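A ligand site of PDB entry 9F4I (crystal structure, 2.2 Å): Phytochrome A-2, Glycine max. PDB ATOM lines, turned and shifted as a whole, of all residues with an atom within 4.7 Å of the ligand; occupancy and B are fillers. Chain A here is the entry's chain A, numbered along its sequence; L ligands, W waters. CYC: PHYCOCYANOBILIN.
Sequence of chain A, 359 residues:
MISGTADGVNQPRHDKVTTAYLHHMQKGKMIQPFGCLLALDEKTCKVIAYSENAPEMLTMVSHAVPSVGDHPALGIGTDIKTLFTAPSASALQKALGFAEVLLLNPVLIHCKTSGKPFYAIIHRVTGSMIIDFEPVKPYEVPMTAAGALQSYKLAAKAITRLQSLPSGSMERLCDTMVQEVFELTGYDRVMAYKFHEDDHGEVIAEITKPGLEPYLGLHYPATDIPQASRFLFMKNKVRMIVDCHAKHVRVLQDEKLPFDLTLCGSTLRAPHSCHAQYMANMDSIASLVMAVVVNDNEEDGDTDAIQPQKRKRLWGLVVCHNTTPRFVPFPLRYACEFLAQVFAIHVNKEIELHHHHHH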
ATOM      1  N   TYR A 193      13.834  27.075  14.031  1.00  0.00           N
ATOM      2  CA  TYR A 193      13.497  28.373  13.458  1.00  0.00           C
ATOM      3  C   TYR A 193      14.272  29.454  14.206  1.00  0.00           C
ATOM      4  O   TYR A 193      14.355  29.429  15.442  1.00  0.00           O
ATOM      5  CB  TYR A 193      12.007  28.648  13.514  1.00  0.00           C
ATOM      6  CG  TYR A 193      11.172  27.705  12.676  1.00  0.00           C
ATOM      7  CD1 TYR A 193      11.645  27.176  11.483  1.00  0.00           C
ATOM      8  CD2 TYR A 193       9.906  27.352  13.071  1.00  0.00           C
ATOM      9  CE1 TYR A 193      10.867  26.309  10.724  1.00  0.00           C
ATOM     10  CE2 TYR A 193       9.137  26.506  12.336  1.00  0.00           C
ATOM     11  CZ  TYR A 193       9.612  25.993  11.162  1.00  0.00           C
ATOM     12  OH  TYR A 193       8.800  25.140  10.448  1.00  0.00           O
ATOM     13  N   TYR A 220      10.919  32.725   5.747  1.00  0.00           N
ATOM     14  CA  TYR A 220       9.491  32.891   5.574  1.00  0.00           C
ATOM     15  C   TYR A 220       9.000  34.135   6.292  1.00  0.00           C
ATOM     16  O   TYR A 220       9.591  34.543   7.305  1.00  0.00           O
ATOM     17  CB  TYR A 220       8.702  31.657   6.028  1.00  0.00           C
ATOM     18  CG  TYR A 220       8.903  31.216   7.456  1.00  0.00           C
ATOM     19  CD1 TYR A 220       8.102  31.706   8.488  1.00  0.00           C
ATOM     20  CD2 TYR A 220       9.843  30.244   7.761  1.00  0.00           C
ATOM     21  CE1 TYR A 220       8.259  31.273   9.790  1.00  0.00           C
ATOM     22  CE2 TYR A 220      10.006  29.803   9.064  1.00  0.00           C
ATOM     23  CZ  TYR A 220       9.213  30.323  10.074  1.00  0.00           C
ATOM     24  OH  TYR A 220       9.391  29.880  11.360  1.00  0.00           O
ATOM     25  N   THR A 223       4.373  37.317   8.954  1.00  0.00           N
ATOM     26  CA  THR A 223       2.928  37.124   9.099  1.00  0.00           C
ATOM     27  C   THR A 223       2.523  35.648   9.083  1.00  0.00           C
ATOM     28  O   THR A 223       1.347  35.341   9.318  1.00  0.00           O
ATOM     29  CB  THR A 223       2.160  37.881   7.987  1.00  0.00           C
ATOM     30  OG1 THR A 223       2.389  37.257   6.717  1.00  0.00           O
ATOM     31  CG2 THR A 223       2.591  39.347   7.943  1.00  0.00           C
ATOM     32  N   ASP A 224       3.462  34.724   8.825  1.00  0.00           N
ATOM     33  CA  ASP A 224       3.116  33.313   8.897  1.00  0.00           C
ATOM     34  C   ASP A 224       2.843  32.870  10.325  1.00  0.00           C
ATOM     35  O   ASP A 224       2.166  31.844  10.519  1.00  0.00           O
ATOM     36  CB  ASP A 224       4.225  32.447   8.312  1.00  0.00           C
ATOM     37  CG  ASP A 224       4.429  32.680   6.848  1.00  0.00           C
ATOM     38  OD1 ASP A 224       3.661  33.475   6.268  1.00  0.00           O
ATOM     39  OD2 ASP A 224       5.368  32.091   6.280  1.00  0.00           O
ATOM     40  N   ILE A 225       3.362  33.589  11.311  1.00  0.00           N
ATOM     41  CA  ILE A 225       3.117  33.307  12.725  1.00  0.00           C
ATOM     42  C   ILE A 225       2.680  34.615  13.387  1.00  0.00           C
ATOM     43  O   ILE A 225       3.520  35.483  13.649  1.00  0.00           O
ATOM     44  CB  ILE A 225       4.359  32.714  13.422  1.00  0.00           C
ATOM     45  CG1 ILE A 225       4.894  31.500  12.654  1.00  0.00           C
ATOM     46  CG2 ILE A 225       4.055  32.324  14.851  1.00  0.00           C
ATOM     47  CD1 ILE A 225       6.288  31.118  13.019  1.00  0.00           C
ATOM     48  N   PRO A 226       1.390  34.794  13.656  1.00  0.00           N
ATOM     49  CA  PRO A 226       0.915  36.032  14.286  1.00  0.00           C
ATOM     50  C   PRO A 226       1.458  36.203  15.700  1.00  0.00           C
ATOM     51  O   PRO A 226       1.812  35.230  16.369  1.00  0.00           O
ATOM     52  CB  PRO A 226      -0.603  35.863  14.307  1.00  0.00           C
ATOM     53  CG  PRO A 226      -0.815  34.368  14.243  1.00  0.00           C
ATOM     54  CD  PRO A 226       0.274  33.885  13.342  1.00  0.00           C
ATOM     55  N   SER A 229       0.170  34.106  18.641  1.00  0.00           N
ATOM     56  CA  SER A 229       0.634  32.730  18.700  1.00  0.00           C
ATOM     57  C   SER A 229       2.044  32.640  19.255  1.00  0.00           C
ATOM     58  O   SER A 229       2.434  31.611  19.806  1.00  0.00           O
ATOM     59  CB  SER A 229       0.554  32.072  17.317  1.00  0.00           C
ATOM     60  OG  SER A 229      -0.742  32.200  16.753  1.00  0.00           O
ATOM     61  N   PHE A 233       3.153  30.435  22.517  1.00  0.00           N
ATOM     62  CA  PHE A 233       4.373  29.645  22.476  1.00  0.00           C
ATOM     63  C   PHE A 233       5.301  29.972  23.649  1.00  0.00           C
ATOM     64  O   PHE A 233       5.964  29.078  24.177  1.00  0.00           O
ATOM     65  CB  PHE A 233       5.100  29.877  21.144  1.00  0.00           C
ATOM     66  CG  PHE A 233       4.497  29.142  19.955  1.00  0.00           C
ATOM     67  CD1 PHE A 233       3.900  27.910  20.133  1.00  0.00           C
ATOM     68  CD2 PHE A 233       4.557  29.682  18.673  1.00  0.00           C
ATOM     69  CE1 PHE A 233       3.359  27.232  19.055  1.00  0.00           C
ATOM     70  CE2 PHE A 233       4.017  29.003  17.595  1.00  0.00           C
ATOM     71  CZ  PHE A 233       3.427  27.780  17.792  1.00  0.00           C
ATOM     72  N   ARG A 239       4.060  22.764  23.106  1.00  0.00           N
ATOM     73  CA  ARG A 239       2.720  22.554  22.569  1.00  0.00           C
ATOM     74  C   ARG A 239       2.751  21.401  21.582  1.00  0.00           C
ATOM     75  O   ARG A 239       3.733  21.204  20.875  1.00  0.00           O
ATOM     76  CB  ARG A 239       2.176  23.821  21.865  1.00  0.00           C
ATOM     77  CG  ARG A 239       1.103  24.560  22.614  1.00  0.00           C
ATOM     78  CD  ARG A 239       0.328  25.613  21.811  1.00  0.00           C
ATOM     79  NE  ARG A 239      -0.582  25.082  20.790  1.00  0.00           N
ATOM     80  CZ  ARG A 239      -1.800  24.603  21.028  1.00  0.00           C
ATOM     81  NH1 ARG A 239      -2.272  24.499  22.253  1.00  0.00           N
ATOM     82  NH2 ARG A 239      -2.543  24.202  20.008  1.00  0.00           N
ATOM     83  N   ILE A 241       0.399  19.067  18.632  1.00  0.00           N
ATOM     84  CA  ILE A 241      -0.733  18.855  17.744  1.00  0.00           C
ATOM     85  C   ILE A 241      -0.663  17.401  17.288  1.00  0.00           C
ATOM     86  O   ILE A 241       0.353  16.963  16.753  1.00  0.00           O
ATOM     87  CB  ILE A 241      -0.709  19.805  16.534  1.00  0.00           C
ATOM     88  CG1 ILE A 241      -0.659  21.265  17.007  1.00  0.00           C
ATOM     89  CG2 ILE A 241      -1.935  19.585  15.677  1.00  0.00           C
ATOM     90  CD1 ILE A 241      -0.699  22.247  15.881  1.00  0.00           C
ATOM     91  N   ARG A 269      -5.639  22.475  23.907  1.00  0.00           N
ATOM     92  CA  ARG A 269      -6.204  23.553  23.104  1.00  0.00           C
ATOM     93  C   ARG A 269      -6.108  23.267  21.609  1.00  0.00           C
ATOM     94  O   ARG A 269      -5.088  22.759  21.122  1.00  0.00           O
ATOM     95  CB  ARG A 269      -5.511  24.870  23.442  1.00  0.00           C
ATOM     96  CG  ARG A 269      -6.404  26.120  23.303  1.00  0.00           C
ATOM     97  CD  ARG A 269      -5.622  27.429  23.425  1.00  0.00           C
ATOM     98  NE  ARG A 269      -4.557  27.531  22.438  1.00  0.00           N
ATOM     99  CZ  ARG A 269      -3.268  27.350  22.685  1.00  0.00           C
ATOM    100  NH1 ARG A 269      -2.832  27.027  23.888  1.00  0.00           N
ATOM    101  NH2 ARG A 269      -2.381  27.503  21.693  1.00  0.00           N
ATOM    102  N   ALA A 270      -7.177  23.560  20.878  1.00  0.00           N
ATOM    103  CA  ALA A 270      -7.207  23.332  19.441  1.00  0.00           C
ATOM    104  C   ALA A 270      -6.389  24.390  18.696  1.00  0.00           C
ATOM    105  O   ALA A 270      -6.186  25.501  19.190  1.00  0.00           O
ATOM    106  CB  ALA A 270      -8.648  23.338  18.937  1.00  0.00           C
ATOM    107  N   PRO A 271      -5.873  24.062  17.523  1.00  0.00           N
ATOM    108  CA  PRO A 271      -5.230  25.079  16.696  1.00  0.00           C
ATOM    109  C   PRO A 271      -6.274  25.942  16.006  1.00  0.00           C
ATOM    110  O   PRO A 271      -7.423  25.538  15.833  1.00  0.00           O
ATOM    111  CB  PRO A 271      -4.442  24.249  15.672  1.00  0.00           C
ATOM    112  CG  PRO A 271      -5.302  23.040  15.485  1.00  0.00           C
ATOM    113  CD  PRO A 271      -5.899  22.747  16.853  1.00  0.00           C
ATOM    114  N   HIS A 272      -5.865  27.152  15.628  1.00  0.00           N
ATOM    115  CA  HIS A 272      -6.713  27.952  14.760  1.00  0.00           C
ATOM    116  C   HIS A 272      -6.884  27.252  13.420  1.00  0.00           C
ATOM    117  O   HIS A 272      -5.898  26.773  12.831  1.00  0.00           O
ATOM    118  CB  HIS A 272      -6.134  29.347  14.569  1.00  0.00           C
ATOM    119  CG  HIS A 272      -7.141  30.356  14.100  1.00  0.00           C
ATOM    120  ND1 HIS A 272      -7.504  30.473  12.772  1.00  0.00           N
ATOM    121  CD2 HIS A 272      -7.865  31.274  14.762  1.00  0.00           C
ATOM    122  CE1 HIS A 272      -8.404  31.426  12.647  1.00  0.00           C
ATOM    123  NE2 HIS A 272      -8.647  31.932  13.846  1.00  0.00           N
ATOM    124  N   CYS A 274      -6.901  27.989  10.562  1.00  0.00           N
ATOM    125  CA  CYS A 274      -6.047  28.386   9.434  1.00  0.00           C
ATOM    126  C   CYS A 274      -4.753  27.579   9.414  1.00  0.00           C
ATOM    127  O   CYS A 274      -4.273  27.203   8.336  1.00  0.00           O
ATOM    128  CB  CYS A 274      -5.734  29.883   9.504  1.00  0.00           C
ATOM    129  SG  CYS A 274      -4.292  30.394   8.499  1.00  0.00           S
ATOM    130  N   HIS A 275      -4.171  27.330  10.589  1.00  0.00           N
ATOM    131  CA  HIS A 275      -2.925  26.580  10.645  1.00  0.00           C
ATOM    132  C   HIS A 275      -3.128  25.101  10.344  1.00  0.00           C
ATOM    133  O   HIS A 275      -2.236  24.451   9.802  1.00  0.00           O
ATOM    134  CB  HIS A 275      -2.260  26.740  12.013  1.00  0.00           C
ATOM    135  CG  HIS A 275      -1.010  25.949  12.164  1.00  0.00           C
ATOM    136  ND1 HIS A 275       0.138  26.212  11.440  1.00  0.00           N
ATOM    137  CD2 HIS A 275      -0.711  24.878  12.948  1.00  0.00           C
ATOM    138  CE1 HIS A 275       1.080  25.357  11.773  1.00  0.00           C
ATOM    139  NE2 HIS A 275       0.595  24.534  12.678  1.00  0.00           N
ATOM    140  N   TYR A 278      -2.912  24.949   6.565  1.00  0.00           N
ATOM    141  CA  TYR A 278      -1.567  25.114   6.040  1.00  0.00           C
ATOM    142  C   TYR A 278      -0.697  23.894   6.330  1.00  0.00           C
ATOM    143  O   TYR A 278       0.220  23.578   5.560  1.00  0.00           O
ATOM    144  CB  TYR A 278      -0.927  26.382   6.628  1.00  0.00           C
ATOM    145  CG  TYR A 278       0.371  26.830   5.962  1.00  0.00           C
ATOM    146  CD1 TYR A 278       1.592  26.245   6.297  1.00  0.00           C
ATOM    147  CD2 TYR A 278       0.378  27.863   5.031  1.00  0.00           C
ATOM    148  CE1 TYR A 278       2.769  26.667   5.712  1.00  0.00           C
ATOM    149  CE2 TYR A 278       1.570  28.283   4.430  1.00  0.00           C
ATOM    150  CZ  TYR A 278       2.747  27.678   4.782  1.00  0.00           C
ATOM    151  OH  TYR A 278       3.932  28.082   4.207  1.00  0.00           O
ATOM    152  N   MET A 282       1.407  21.151   3.463  1.00  0.00           N
ATOM    153  CA  MET A 282       2.806  20.813   3.680  1.00  0.00           C
ATOM    154  C   MET A 282       3.015  19.345   3.999  1.00  0.00           C
ATOM    155  O   MET A 282       4.150  18.927   4.228  1.00  0.00           O
ATOM    156  CB  MET A 282       3.375  21.671   4.821  1.00  0.00           C
ATOM    157  CG  MET A 282       4.877  21.831   4.849  1.00  0.00           C
ATOM    158  SD  MET A 282       5.339  22.573   6.414  1.00  0.00           S
ATOM    159  CE  MET A 282       3.871  23.519   6.732  1.00  0.00           C
ATOM    160  N   VAL A 289       6.157  21.463  19.297  1.00  0.00           N
ATOM    161  CA  VAL A 289       6.875  22.732  19.218  1.00  0.00           C
ATOM    162  C   VAL A 289       7.445  23.085  20.579  1.00  0.00           C
ATOM    163  O   VAL A 289       6.741  23.014  21.600  1.00  0.00           O
ATOM    164  CB  VAL A 289       5.967  23.867  18.704  1.00  0.00           C
ATOM    165  CG1 VAL A 289       6.713  25.203  18.709  1.00  0.00           C
ATOM    166  CG2 VAL A 289       5.431  23.563  17.307  1.00  0.00           C
ATOM    167  N   LEU A 317      12.486  28.651  17.748  1.00  0.00           N
ATOM    168  CA  LEU A 317      11.713  27.470  18.051  1.00  0.00           C
ATOM    169  C   LEU A 317      12.515  26.261  17.614  1.00  0.00           C
ATOM    170  O   LEU A 317      13.316  26.312  16.684  1.00  0.00           O
ATOM    171  CB  LEU A 317      10.345  27.493  17.344  1.00  0.00           C
ATOM    172  CG  LEU A 317       9.317  28.593  17.661  1.00  0.00           C
ATOM    173  CD1 LEU A 317       8.097  28.413  16.773  1.00  0.00           C
ATOM    174  CD2 LEU A 317       8.916  28.601  19.138  1.00  0.00           C
ATOM    175  N   VAL A 319      11.326  22.518  16.385  1.00  0.00           N
ATOM    176  CA  VAL A 319      10.054  22.079  15.830  1.00  0.00           C
ATOM    177  C   VAL A 319      10.164  20.665  15.303  1.00  0.00           C
ATOM    178  O   VAL A 319      11.116  20.317  14.600  1.00  0.00           O
ATOM    179  CB  VAL A 319       9.571  23.020  14.706  1.00  0.00           C
ATOM    180  CG1 VAL A 319       8.319  22.466  14.075  1.00  0.00           C
ATOM    181  CG2 VAL A 319       9.315  24.412  15.267  1.00  0.00           C
ATOM    182  N   HIS A 321       7.859  18.013  13.082  1.00  0.00           N
ATOM    183  CA  HIS A 321       6.729  17.715  12.224  1.00  0.00           C
ATOM    184  C   HIS A 321       6.791  16.247  11.831  1.00  0.00           C
ATOM    185  O   HIS A 321       7.878  15.676  11.688  1.00  0.00           O
ATOM    186  CB  HIS A 321       6.699  18.555  10.950  1.00  0.00           C
ATOM    187  CG  HIS A 321       6.402  19.994  11.187  1.00  0.00           C
ATOM    188  ND1 HIS A 321       6.424  20.931  10.184  1.00  0.00           N
ATOM    189  CD2 HIS A 321       6.063  20.661  12.320  1.00  0.00           C
ATOM    190  CE1 HIS A 321       6.134  22.114  10.681  1.00  0.00           C
ATOM    191  NE2 HIS A 321       5.908  21.978  11.977  1.00  0.00           N
HETATM  192  CHA CYC L   1       1.994  28.542  13.011  1.00  0.00           C
HETATM  193  NA  CYC L   1       2.821  28.925  10.733  1.00  0.00           N
HETATM  194  C1A CYC L   1       2.976  28.502  12.027  1.00  0.00           C
HETATM  195  C2A CYC L   1       4.353  28.123  12.277  1.00  0.00           C
HETATM  196  C3A CYC L   1       5.012  28.288  11.099  1.00  0.00           C
HETATM  197  C4A CYC L   1       4.010  28.679  10.106  1.00  0.00           C
HETATM  198  CMA CYC L   1       6.499  28.154  10.900  1.00  0.00           C
HETATM  199  CAA CYC L   1       4.922  27.736  13.610  1.00  0.00           C
HETATM  200  CBA CYC L   1       4.610  26.301  14.045  1.00  0.00           C
HETATM  201  CGA CYC L   1       5.479  25.242  13.388  1.00  0.00           C
HETATM  202  O1A CYC L   1       4.917  24.302  12.799  1.00  0.00           O
HETATM  203  O2A CYC L   1       6.706  25.358  13.479  1.00  0.00           O
HETATM  204  CHB CYC L   1       4.257  28.968   8.777  1.00  0.00           C
HETATM  205  NB  CYC L   1       5.536  29.329   6.741  1.00  0.00           N
HETATM  206  C1B CYC L   1       5.169  28.574   7.849  1.00  0.00           C
HETATM  207  C2B CYC L   1       5.734  27.275   7.705  1.00  0.00           C
HETATM  208  C3B CYC L   1       6.673  27.331   6.731  1.00  0.00           C
HETATM  209  C4B CYC L   1       6.537  28.665   6.062  1.00  0.00           C
HETATM  210  CMB CYC L   1       5.432  26.024   8.467  1.00  0.00           C
HETATM  211  CAB CYC L   1       7.675  26.303   6.294  1.00  0.00           C
HETATM  212  CBB CYC L   1       7.149  25.428   5.157  1.00  0.00           C
HETATM  213  OB  CYC L   1       7.129  29.085   5.100  1.00  0.00           O
HETATM  214  NC  CYC L   1      -0.740  30.678   9.322  1.00  0.00           N
HETATM  215  C1C CYC L   1      -0.793  31.039   8.003  1.00  0.00           C
HETATM  216  C2C CYC L   1      -1.915  32.042   7.814  1.00  0.00           C
HETATM  217  C3C CYC L   1      -2.543  32.183   9.206  1.00  0.00           C
HETATM  218  C4C CYC L   1      -1.766  31.226  10.078  1.00  0.00           C
HETATM  219  CMC CYC L   1      -1.480  33.354   7.166  1.00  0.00           C
HETATM  220  CAC CYC L   1      -4.068  31.995   9.217  1.00  0.00           C
HETATM  221  CBC CYC L   1      -4.768  32.784  10.307  1.00  0.00           C
HETATM  222  OC  CYC L   1      -0.051  30.628   7.132  1.00  0.00           O
HETATM  223  CHD CYC L   1      -1.969  30.973  11.430  1.00  0.00           C
HETATM  224  ND  CYC L   1       0.150  29.782  11.947  1.00  0.00           N
HETATM  225  C1D CYC L   1      -1.094  30.245  12.302  1.00  0.00           C
HETATM  226  C2D CYC L   1      -1.333  29.849  13.657  1.00  0.00           C
HETATM  227  C3D CYC L   1      -0.223  29.159  14.086  1.00  0.00           C
HETATM  228  C4D CYC L   1       0.719  29.119  12.999  1.00  0.00           C
HETATM  229  CMD CYC L   1      -2.563  30.137  14.442  1.00  0.00           C
HETATM  230  CAD CYC L   1      -0.016  28.566  15.455  1.00  0.00           C
HETATM  231  CBD CYC L   1      -0.741  27.235  15.627  1.00  0.00           C
HETATM  232  CGD CYC L   1      -1.044  26.871  17.065  1.00  0.00           C
HETATM  233  O1D CYC L   1      -0.119  26.464  17.789  1.00  0.00           O
HETATM  234  O2D CYC L   1      -2.218  26.985  17.468  1.00  0.00           O
HETATM  235  O   HOH W   1       0.718  28.490  20.044  1.00  0.00           O
HETATM  236  O   HOH W   2       0.795  28.443   9.463  1.00  0.00           O
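A nitrogen (ND) of the ligand sits at hydrogen-bond distance from the backbone carbonyl oxygen (O) of Asp 224. OD2 of Asp 224 sits at hydrogen-bond distance from NB of the ligand (2.8 Å). A ring nitrogen (NE2) of His 321 lies within hydrogen-bond range of an oxygen (O1A) of the ligand (2.7 Å). An oxygen (O1D) of the ligand is in salt-bridge range of the guanidinium group (NE) of Arg 239, at 3.3 Å. A carbon (CAC) of the ligand is covalently linked to the side-chain sulfur (SG) of Cys 274, at 1.8 Å. The side-chain hydroxyl (OH) of Tyr 278 lies within hydrogen-bond range of a nitrogen (NB) of the ligand, at 3.2 Å.
N of Val 289 lies within hydrogen-bond range of O of Arg 239, at 2.9 Å. N of Cys 274 sits close to ND1 of His 272, at 3.4 Å. The backbone NH (N) of Tyr 193 sits at hydrogen-bond distance from the backbone carbonyl oxygen (O) of Leu 317 (2.8 Å). O of Arg 269 lies within hydrogen-bond range of NH2 of Arg 239 (3.1 Å).
Merely in contact with the ligand: Tyr 193 (2.9 Å), Tyr 220 (3.2 Å), Ile 225 (3.4 Å), Ser 229 (3.6 Å), Phe 233 (3.8 Å), Pro 271 (3.6 Å), His 272 (3.7 Å), His 275 (3.3 Å), Met 282 (3.4 Å) and Val 319 (3.3 Å). The nearest printed residue that does not touch the ligand is Pro 226 (4.03 Å).
Water W2 bridges a nitrogen (NA) of the ligand (2.4 Å) and a ring nitrogen (ND1) of His 275 (3.1 Å).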
